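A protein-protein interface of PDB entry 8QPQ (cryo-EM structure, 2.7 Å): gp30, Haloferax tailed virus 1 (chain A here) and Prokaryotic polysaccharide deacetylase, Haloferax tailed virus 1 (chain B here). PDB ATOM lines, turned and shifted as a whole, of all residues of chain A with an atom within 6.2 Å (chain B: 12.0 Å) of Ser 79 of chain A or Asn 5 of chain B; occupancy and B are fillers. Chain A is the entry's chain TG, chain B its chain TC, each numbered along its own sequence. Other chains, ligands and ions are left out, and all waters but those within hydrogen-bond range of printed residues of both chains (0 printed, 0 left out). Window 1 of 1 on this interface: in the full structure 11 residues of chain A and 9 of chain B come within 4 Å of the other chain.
O3P of NEP 45 of chain A is in hydrogen-bond range of N of Ile 78 of chain A (2.9 Å).
The side-chain amide nitrogen (ND2) of Asn 5 of chain B lies within hydrogen-bond range of the backbone carbonyl oxygen (O) of Thr 12 of chain B (3.3 Å).
The backbone carbonyl oxygen of His 41 of chain A sits at hydrogen-bond distance from the backbone NH of Asn 82 of chain A (2.9 Å).
N of NEP 45 of chain A lies within hydrogen-bond range of O of Gly 77 of chain A.
OG of Ser 79 of chain A sits at hydrogen-bond distance from ND2 of Asn 82 of chain A, 2.9 Å away.
The side-chain amide oxygen of Asn 42 of chain A is in hydrogen-bond range of the backbone NH of Gly 81 of chain A, 3.5 Å away.
Of the 13 printed residues of chain A, 9 touch a printed residue of chain B.
Hydrophobic or aromatic side chains of chain A within 4 Å of the printed part of chain B: Phe 73 and Ile 78.
Of the 17 printed residues of chain B, 9 touch a printed residue of chain A.
Among the printed residues, pairs that only touch across the chains: Asp 71 of chain A with Gly 3 of chain B (3.7 Å), Phe 73 of chain A with Leu 4 of chain B (3.6 Å), Gly 77 of chain A with Asp 7 of chain B (3.6 Å), Ile 78 of chain A with Pro 6 of chain B (3.7 Å), Ile 78 of chain A with Asp 7 of chain B (3.4 Å), Ile 78 of chain A with Leu 9 of chain B (3.6 Å), Gln 80 of chain A with Gly 8 of chain B (3.5 Å), Gln 80 of chain A with Leu 9 of chain B (3.5 Å) and Asn 82 of chain A with Leu 4 of chain B (3.5 Å).
No residue of chain B comes within 4 Å of Asn 42 of chain A.
Ile 43 of chain A touches none of the printed residues of chain B.
No residue of chain B comes within 4 Å of Ala 44 of chain A.
Of the printed residues of chain B, Asp 71 of chain A touches Gly 3 (3.7 Å) and Leu 4 (2.9 Å).
Gly 77 of chain A touches one residue of chain B.
Ser 79 of chain A touches just one residue of chain B: Asn 5 (2.6 Å).
Of chain B, only Asn 5 (3.1 Å) comes within 4 Å of Gly 81 of chain A.
Printed residues of chain A within 4 Å of Gly 3 of chain B: Asp 71 (3.7 Å).
Of the printed residues of chain A, Gly 8 of chain B touches Ile 78 and Gln 80.
The nearest residue of chain B that does not touch Ser 79 of chain A is Pro 6 of chain B (4.1 Å).
The nearest residue of chain A that does not touch Asn 5 of chain B is Phe 73 of chain A (4.3 Å).
The nearest printed residue of chain A that does not touch Leu 4 of chain B is Ser 79 of chain A (4.2 Å).
The side-chain hydroxyl of Thr 12 of chain B sits at hydrogen-bond distance from the backbone carbonyl oxygen of Gln 80 of chain A, 3.3 Å away.
The backbone NH of Asn 5 of chain B sits at hydrogen-bond distance from the side-chain amide oxygen of Asn 82 of chain A (2.8 Å).
The backbone carbonyl oxygen of Gly 81 of chain A sits at hydrogen-bond distance from the side-chain amide nitrogen of Asn 5 of chain B (3.1 Å).
O of Ile 78 of chain A sits at hydrogen-bond distance from N of Gly 8 of chain B.
N of Leu 4 of chain B sits at hydrogen-bond distance from OD2 of Asp 71 of chain A.
O3P of NEP 45 of chain A sits close to the side-chain carboxylate of Asp 7 of chain B.
OG of Ser 79 of chain A is in hydrogen-bond range of O of Asn 5 of chain B (2.6 Å).
O of Gly 10 of chain B lies within hydrogen-bond range of NE2 of Gln 80 of chain A, 2.8 Å away.
ND2 of Asn 5 of chain B sits at hydrogen-bond distance from O of Gln 80 of chain A (2.6 Å).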
ATOM      1  N   HIS A  41      15.497  11.889 -19.821  1.00  0.00           N
ATOM      2  CA  HIS A  41      14.441  11.009 -20.286  1.00  0.00           C
ATOM      3  C   HIS A  41      13.190  11.194 -19.428  1.00  0.00           C
ATOM      4  O   HIS A  41      12.087  11.315 -19.944  1.00  0.00           O
ATOM      5  CB  HIS A  41      14.922   9.556 -20.209  1.00  0.00           C
ATOM      6  CG  HIS A  41      16.121   9.253 -21.048  1.00  0.00           C
ATOM      7  ND1 HIS A  41      16.891   8.099 -20.878  1.00  0.00           N
ATOM      8  CD2 HIS A  41      16.658   9.931 -22.085  1.00  0.00           C
ATOM      9  CE1 HIS A  41      17.850   8.096 -21.774  1.00  0.00           C
ATOM     10  NE2 HIS A  41      17.723   9.212 -22.533  1.00  0.00           N
ATOM     11  N   ASN A  42      13.402  11.271 -18.114  1.00  0.00           N
ATOM     12  CA  ASN A  42      12.333  11.195 -17.148  1.00  0.00           C
ATOM     13  C   ASN A  42      12.300  12.461 -16.305  1.00  0.00           C
ATOM     14  O   ASN A  42      13.324  12.904 -15.797  1.00  0.00           O
ATOM     15  CB  ASN A  42      12.595  10.023 -16.219  1.00  0.00           C
ATOM     16  CG  ASN A  42      12.639   8.684 -16.913  1.00  0.00           C
ATOM     17  OD1 ASN A  42      12.045   8.421 -17.953  1.00  0.00           O
ATOM     18  ND2 ASN A  42      13.424   7.800 -16.347  1.00  0.00           N
ATOM     19  N   ILE A  43      11.099  13.022 -16.151  1.00  0.00           N
ATOM     20  CA  ILE A  43      10.836  14.037 -15.148  1.00  0.00           C
ATOM     21  C   ILE A  43       9.667  13.533 -14.304  1.00  0.00           C
ATOM     22  O   ILE A  43       8.529  13.475 -14.771  1.00  0.00           O
ATOM     23  CB  ILE A  43      10.541  15.398 -15.821  1.00  0.00           C
ATOM     24  CG1 ILE A  43      11.774  15.898 -16.585  1.00  0.00           C
ATOM     25  CG2 ILE A  43      10.032  16.411 -14.796  1.00  0.00           C
ATOM     26  CD1 ILE A  43      11.561  17.117 -17.444  1.00  0.00           C
ATOM     27  N   ALA A  44       9.960  13.139 -13.069  1.00  0.00           N
ATOM     28  CA  ALA A  44       8.970  12.744 -12.084  1.00  0.00           C
ATOM     29  C   ALA A  44       8.769  13.935 -11.158  1.00  0.00           C
ATOM     30  O   ALA A  44       9.724  14.365 -10.516  1.00  0.00           O
ATOM     31  CB  ALA A  44       9.478  11.510 -11.350  1.00  0.00           C
ATOM     32  N   NEP A  45       7.551  14.473 -11.034  1.00  0.00           N
ATOM     33  CA  NEP A  45       7.439  15.868 -10.629  1.00  0.00           C
ATOM     34  C   NEP A  45       6.677  16.155  -9.326  1.00  0.00           C
ATOM     35  O   NEP A  45       6.794  17.278  -8.828  1.00  0.00           O
ATOM     36  CB  NEP A  45       6.952  16.726 -11.816  1.00  0.00           C
ATOM     37  CG  NEP A  45       5.760  16.251 -12.585  1.00  0.00           C
ATOM     38  ND1 NEP A  45       4.446  16.596 -12.261  1.00  0.00           N
ATOM     39  CD2 NEP A  45       5.732  15.509 -13.726  1.00  0.00           C
ATOM     40  CE1 NEP A  45       3.697  16.083 -13.221  1.00  0.00           C
ATOM     41  NE2 NEP A  45       4.401  15.401 -14.169  1.00  0.00           N
ATOM     42  P   NEP A  45       3.804  14.687 -15.653  1.00  0.00           P
ATOM     43  O1P NEP A  45       2.614  15.554 -16.058  1.00  0.00           O
ATOM     44  O2P NEP A  45       4.960  14.858 -16.569  1.00  0.00           O
ATOM     45  O3P NEP A  45       3.460  13.297 -15.267  1.00  0.00           O
ATOM     46  N   ASP A  71       7.278  22.554 -21.926  1.00  0.00           N
ATOM     47  CA  ASP A  71       5.957  22.031 -21.617  1.00  0.00           C
ATOM     48  C   ASP A  71       5.560  22.356 -20.179  1.00  0.00           C
ATOM     49  O   ASP A  71       6.409  22.678 -19.343  1.00  0.00           O
ATOM     50  CB  ASP A  71       5.892  20.521 -21.869  1.00  0.00           C
ATOM     51  CG  ASP A  71       4.550  20.038 -22.412  1.00  0.00           C
ATOM     52  OD1 ASP A  71       3.545  20.769 -22.281  1.00  0.00           O
ATOM     53  OD2 ASP A  71       4.525  18.929 -23.010  1.00  0.00           O
ATOM     54  N   PHE A  73       3.412  20.550 -16.988  1.00  0.00           N
ATOM     55  CA  PHE A  73       2.914  19.301 -16.442  1.00  0.00           C
ATOM     56  C   PHE A  73       2.028  19.612 -15.240  1.00  0.00           C
ATOM     57  O   PHE A  73       2.354  20.492 -14.440  1.00  0.00           O
ATOM     58  CB  PHE A  73       4.135  18.506 -15.987  1.00  0.00           C
ATOM     59  CG  PHE A  73       5.078  18.022 -17.069  1.00  0.00           C
ATOM     60  CD1 PHE A  73       4.686  17.830 -18.392  1.00  0.00           C
ATOM     61  CD2 PHE A  73       6.399  17.749 -16.748  1.00  0.00           C
ATOM     62  CE1 PHE A  73       5.593  17.377 -19.343  1.00  0.00           C
ATOM     63  CE2 PHE A  73       7.289  17.222 -17.673  1.00  0.00           C
ATOM     64  CZ  PHE A  73       6.892  17.080 -18.983  1.00  0.00           C
ATOM     65  N   GLY A  77       3.046  13.012 -11.350  1.00  0.00           N
ATOM     66  CA  GLY A  77       3.267  11.946 -12.309  1.00  0.00           C
ATOM     67  C   GLY A  77       4.698  11.933 -12.825  1.00  0.00           C
ATOM     68  O   GLY A  77       5.588  12.514 -12.241  1.00  0.00           O
ATOM     69  N   ILE A  78       4.887  11.215 -13.939  1.00  0.00           N
ATOM     70  CA  ILE A  78       6.150  11.162 -14.649  1.00  0.00           C
ATOM     71  C   ILE A  78       5.939  11.386 -16.149  1.00  0.00           C
ATOM     72  O   ILE A  78       5.209  10.645 -16.825  1.00  0.00           O
ATOM     73  CB  ILE A  78       6.924   9.860 -14.340  1.00  0.00           C
ATOM     74  CG1 ILE A  78       8.302   9.851 -15.001  1.00  0.00           C
ATOM     75  CG2 ILE A  78       6.112   8.623 -14.708  1.00  0.00           C
ATOM     76  CD1 ILE A  78       9.200   8.736 -14.450  1.00  0.00           C
ATOM     77  N   SER A  79       6.716  12.314 -16.714  1.00  0.00           N
ATOM     78  CA  SER A  79       6.970  12.322 -18.149  1.00  0.00           C
ATOM     79  C   SER A  79       8.160  11.421 -18.410  1.00  0.00           C
ATOM     80  O   SER A  79       9.199  11.661 -17.866  1.00  0.00           O
ATOM     81  CB  SER A  79       7.202  13.725 -18.669  1.00  0.00           C
ATOM     82  OG  SER A  79       7.263  13.668 -20.078  1.00  0.00           O
ATOM     83  N   GLN A  80       7.959  10.349 -19.186  1.00  0.00           N
ATOM     84  CA  GLN A  80       8.936   9.284 -19.358  1.00  0.00           C
ATOM     85  C   GLN A  80       9.358   9.203 -20.827  1.00  0.00           C
ATOM     86  O   GLN A  80       8.556   9.406 -21.739  1.00  0.00           O
ATOM     87  CB  GLN A  80       8.315   7.964 -18.871  1.00  0.00           C
ATOM     88  CG  GLN A  80       9.094   6.710 -19.198  1.00  0.00           C
ATOM     89  CD  GLN A  80       8.529   5.500 -18.505  1.00  0.00           C
ATOM     90  OE1 GLN A  80       9.218   4.826 -17.741  1.00  0.00           O
ATOM     91  NE2 GLN A  80       7.268   5.202 -18.782  1.00  0.00           N
ATOM     92  N   GLY A  81      10.648   8.894 -21.086  1.00  0.00           N
ATOM     93  CA  GLY A  81      11.129   8.575 -22.431  1.00  0.00           C
ATOM     94  C   GLY A  81      11.307   9.780 -23.361  1.00  0.00           C
ATOM     95  O   GLY A  81      11.277   9.646 -24.576  1.00  0.00           O
ATOM     96  N   ASN A  82      11.517  10.959 -22.781  1.00  0.00           N
ATOM     97  CA  ASN A  82      11.918  12.158 -23.509  1.00  0.00           C
ATOM     98  C   ASN A  82      13.371  12.076 -24.003  1.00  0.00           C
ATOM     99  O   ASN A  82      14.108  11.164 -23.675  1.00  0.00           O
ATOM    100  CB  ASN A  82      11.728  13.365 -22.600  1.00  0.00           C
ATOM    101  CG  ASN A  82      10.272  13.576 -22.264  1.00  0.00           C
ATOM    102  OD1 ASN A  82       9.447  13.912 -23.105  1.00  0.00           O
ATOM    103  ND2 ASN A  82       9.939  13.343 -21.020  1.00  0.00           N
ATOM    104  N   THR B   2       5.311  19.771 -30.675  1.00  0.00           N
ATOM    105  CA  THR B   2       5.126  18.343 -30.287  1.00  0.00           C
ATOM    106  C   THR B   2       4.900  18.229 -28.781  1.00  0.00           C
ATOM    107  O   THR B   2       4.024  17.480 -28.363  1.00  0.00           O
ATOM    108  CB  THR B   2       6.328  17.496 -30.712  1.00  0.00           C
ATOM    109  OG1 THR B   2       6.517  17.728 -32.110  1.00  0.00           O
ATOM    110  CG2 THR B   2       6.122  16.016 -30.482  1.00  0.00           C
ATOM    111  N   GLY B   3       5.688  18.980 -27.999  1.00  0.00           N
ATOM    112  CA  GLY B   3       5.680  18.910 -26.544  1.00  0.00           C
ATOM    113  C   GLY B   3       6.480  17.719 -26.012  1.00  0.00           C
ATOM    114  O   GLY B   3       7.089  16.972 -26.782  1.00  0.00           O
ATOM    115  N   LEU B   4       6.463  17.556 -24.683  1.00  0.00           N
ATOM    116  CA  LEU B   4       7.110  16.425 -24.027  1.00  0.00           C
ATOM    117  C   LEU B   4       6.116  15.275 -23.855  1.00  0.00           C
ATOM    118  O   LEU B   4       4.906  15.445 -24.034  1.00  0.00           O
ATOM    119  CB  LEU B   4       7.704  16.869 -22.688  1.00  0.00           C
ATOM    120  CG  LEU B   4       8.752  17.978 -22.773  1.00  0.00           C
ATOM    121  CD1 LEU B   4       9.199  18.407 -21.392  1.00  0.00           C
ATOM    122  CD2 LEU B   4       9.937  17.540 -23.616  1.00  0.00           C
ATOM    123  N   ASN B   5       6.634  14.088 -23.521  1.00  0.00           N
ATOM    124  CA  ASN B   5       5.827  12.878 -23.450  1.00  0.00           C
ATOM    125  C   ASN B   5       4.733  13.008 -22.385  1.00  0.00           C
ATOM    126  O   ASN B   5       4.952  13.614 -21.340  1.00  0.00           O
ATOM    127  CB  ASN B   5       6.711  11.661 -23.194  1.00  0.00           C
ATOM    128  CG  ASN B   5       7.407  11.140 -24.432  1.00  0.00           C
ATOM    129  OD1 ASN B   5       7.173  11.614 -25.534  1.00  0.00           O
ATOM    130  ND2 ASN B   5       8.279  10.164 -24.255  1.00  0.00           N
ATOM    131  N   PRO B   6       3.512  12.462 -22.619  1.00  0.00           N
ATOM    132  CA  PRO B   6       2.453  12.477 -21.611  1.00  0.00           C
ATOM    133  C   PRO B   6       2.847  11.820 -20.296  1.00  0.00           C
ATOM    134  O   PRO B   6       3.727  10.962 -20.236  1.00  0.00           O
ATOM    135  CB  PRO B   6       1.337  11.641 -22.253  1.00  0.00           C
ATOM    136  CG  PRO B   6       1.553  11.820 -23.736  1.00  0.00           C
ATOM    137  CD  PRO B   6       3.059  11.864 -23.888  1.00  0.00           C
ATOM    138  N   ASP B   7       2.166  12.261 -19.243  1.00  0.00           N
ATOM    139  CA  ASP B   7       2.193  11.669 -17.918  1.00  0.00           C
ATOM    140  C   ASP B   7       1.891  10.173 -18.007  1.00  0.00           C
ATOM    141  O   ASP B   7       0.882   9.777 -18.586  1.00  0.00           O
ATOM    142  CB  ASP B   7       1.178  12.416 -17.050  1.00  0.00           C
ATOM    143  CG  ASP B   7       0.897  11.862 -15.659  1.00  0.00           C
ATOM    144  OD1 ASP B   7       1.508  10.842 -15.263  1.00  0.00           O
ATOM    145  OD2 ASP B   7       0.065  12.476 -14.955  1.00  0.00           O
ATOM    146  N   GLY B   8       2.766   9.355 -17.413  1.00  0.00           N
ATOM    147  CA  GLY B   8       2.424   7.973 -17.144  1.00  0.00           C
ATOM    148  C   GLY B   8       3.616   7.042 -17.281  1.00  0.00           C
ATOM    149  O   GLY B   8       4.605   7.354 -17.935  1.00  0.00           O
ATOM    150  N   LEU B   9       3.476   5.872 -16.668  1.00  0.00           N
ATOM    151  CA  LEU B   9       4.349   4.758 -16.974  1.00  0.00           C
ATOM    152  C   LEU B   9       3.791   3.956 -18.150  1.00  0.00           C
ATOM    153  O   LEU B   9       2.791   4.350 -18.755  1.00  0.00           O
ATOM    154  CB  LEU B   9       4.514   3.935 -15.701  1.00  0.00           C
ATOM    155  CG  LEU B   9       5.295   4.634 -14.599  1.00  0.00           C
ATOM    156  CD1 LEU B   9       5.452   3.690 -13.428  1.00  0.00           C
ATOM    157  CD2 LEU B   9       6.657   5.070 -15.109  1.00  0.00           C
ATOM    158  N   GLY B  10       4.499   2.881 -18.508  1.00  0.00           N
ATOM    159  CA  GLY B  10       4.330   2.238 -19.796  1.00  0.00           C
ATOM    160  C   GLY B  10       4.948   3.078 -20.911  1.00  0.00           C
ATOM    161  O   GLY B  10       5.451   4.177 -20.676  1.00  0.00           O
ATOM    162  N   ARG B  11       4.886   2.557 -22.139  1.00  0.00           N
ATOM    163  CA  ARG B  11       5.327   3.293 -23.310  1.00  0.00           C
ATOM    164  C   ARG B  11       4.428   4.518 -23.519  1.00  0.00           C
ATOM    165  O   ARG B  11       3.241   4.388 -23.773  1.00  0.00           O
ATOM    166  CB  ARG B  11       5.318   2.342 -24.509  1.00  0.00           C
ATOM    167  CG  ARG B  11       6.103   2.835 -25.713  1.00  0.00           C
ATOM    168  CD  ARG B  11       6.161   1.748 -26.765  1.00  0.00           C
ATOM    169  NE  ARG B  11       6.537   2.277 -28.066  1.00  0.00           N
ATOM    170  CZ  ARG B  11       6.693   1.551 -29.164  1.00  0.00           C
ATOM    171  NH1 ARG B  11       7.036   2.142 -30.297  1.00  0.00           N
ATOM    172  NH2 ARG B  11       6.508   0.240 -29.142  1.00  0.00           N
ATOM    173  N   THR B  12       5.013   5.712 -23.381  1.00  0.00           N
ATOM    174  CA  THR B  12       4.322   6.971 -23.604  1.00  0.00           C
ATOM    175  C   THR B  12       5.035   7.709 -24.733  1.00  0.00           C
ATOM    176  O   THR B  12       6.266   7.644 -24.839  1.00  0.00           O
ATOM    177  CB  THR B  12       4.278   7.837 -22.336  1.00  0.00           C
ATOM    178  OG1 THR B  12       5.610   7.961 -21.816  1.00  0.00           O
ATOM    179  CG2 THR B  12       3.384   7.254 -21.269  1.00  0.00           C
ATOM    180  N   ALA B  13       4.260   8.421 -25.566  1.00  0.00           N
ATOM    181  CA  ALA B  13       4.857   9.139 -26.680  1.00  0.00           C
ATOM    182  C   ALA B  13       4.103  10.427 -27.000  1.00  0.00           C
ATOM    183  O   ALA B  13       2.877  10.448 -27.018  1.00  0.00           O
ATOM    184  CB  ALA B  13       4.931   8.243 -27.886  1.00  0.00           C
ATOM    185  N   ALA B  14       4.868  11.495 -27.267  1.00  0.00           N
ATOM    186  CA  ALA B  14       4.355  12.706 -27.880  1.00  0.00           C
ATOM    187  C   ALA B  14       4.705  12.693 -29.368  1.00  0.00           C
ATOM    188  O   ALA B  14       5.879  12.664 -29.739  1.00  0.00           O
ATOM    189  CB  ALA B  14       4.931  13.908 -27.169  1.00  0.00           C
ATOM    190  N   PHE B  15       3.666  12.733 -30.205  1.00  0.00           N
ATOM    191  CA  PHE B  15       3.813  12.744 -31.646  1.00  0.00           C
ATOM    192  C   PHE B  15       3.350  14.075 -32.217  1.00  0.00           C
ATOM    193  O   PHE B  15       2.580  14.816 -31.607  1.00  0.00           O
ATOM    194  CB  PHE B  15       2.938  11.657 -32.264  1.00  0.00           C
ATOM    195  CG  PHE B  15       3.336  10.248 -31.913  1.00  0.00           C
ATOM    196  CD1 PHE B  15       4.412   9.638 -32.546  1.00  0.00           C
ATOM    197  CD2 PHE B  15       2.629   9.526 -30.962  1.00  0.00           C
ATOM    198  CE1 PHE B  15       4.765   8.330 -32.246  1.00  0.00           C
ATOM    199  CE2 PHE B  15       2.976   8.212 -30.671  1.00  0.00           C
ATOM    200  CZ  PHE B  15       4.053   7.621 -31.301  1.00  0.00           C
ATOM    201  N   SER B  16       3.821  14.348 -33.430  1.00  0.00           N
ATOM    202  CA  SER B  16       3.169  15.331 -34.267  1.00  0.00           C
ATOM    203  C   SER B  16       2.070  14.622 -35.051  1.00  0.00           C
ATOM    204  O   SER B  16       0.939  14.526 -34.584  1.00  0.00           O
ATOM    205  CB  SER B  16       4.173  16.038 -35.128  1.00  0.00           C
ATOM    206  OG  SER B  16       5.150  16.636 -34.294  1.00  0.00           O
ATOM    207  N   ASN B  17       2.423  14.038 -36.197  1.00  0.00           N
ATOM    208  CA  ASN B  17       1.462  13.387 -37.067  1.00  0.00           C
ATOM    209  C   ASN B  17       1.658  11.868 -37.005  1.00  0.00           C
ATOM    210  O   ASN B  17       2.770  11.372 -37.193  1.00  0.00           O
ATOM    211  CB  ASN B  17       1.531  13.990 -38.472  1.00  0.00           C
ATOM    212  CG  ASN B  17       1.382  15.497 -38.486  1.00  0.00           C
ATOM    213  OD1 ASN B  17       0.676  16.061 -37.659  1.00  0.00           O
ATOM    214  ND2 ASN B  17       2.015  16.159 -39.442  1.00  0.00           N
ATOM    215  N   THR B  18       0.562  11.136 -36.756  1.00  0.00           N
ATOM    216  CA  THR B  18       0.578   9.683 -36.812  1.00  0.00           C
ATOM    217  C   THR B  18      -0.421   9.180 -37.847  1.00  0.00           C
ATOM    218  O   THR B  18      -1.467   9.779 -38.078  1.00  0.00           O
ATOM    219  CB  THR B  18       0.323   9.024 -35.450  1.00  0.00           C
ATOM    220  OG1 THR B  18      -0.988   9.339 -34.979  1.00  0.00           O
ATOM    221  CG2 THR B  18       1.379   9.372 -34.427  1.00  0.00           C
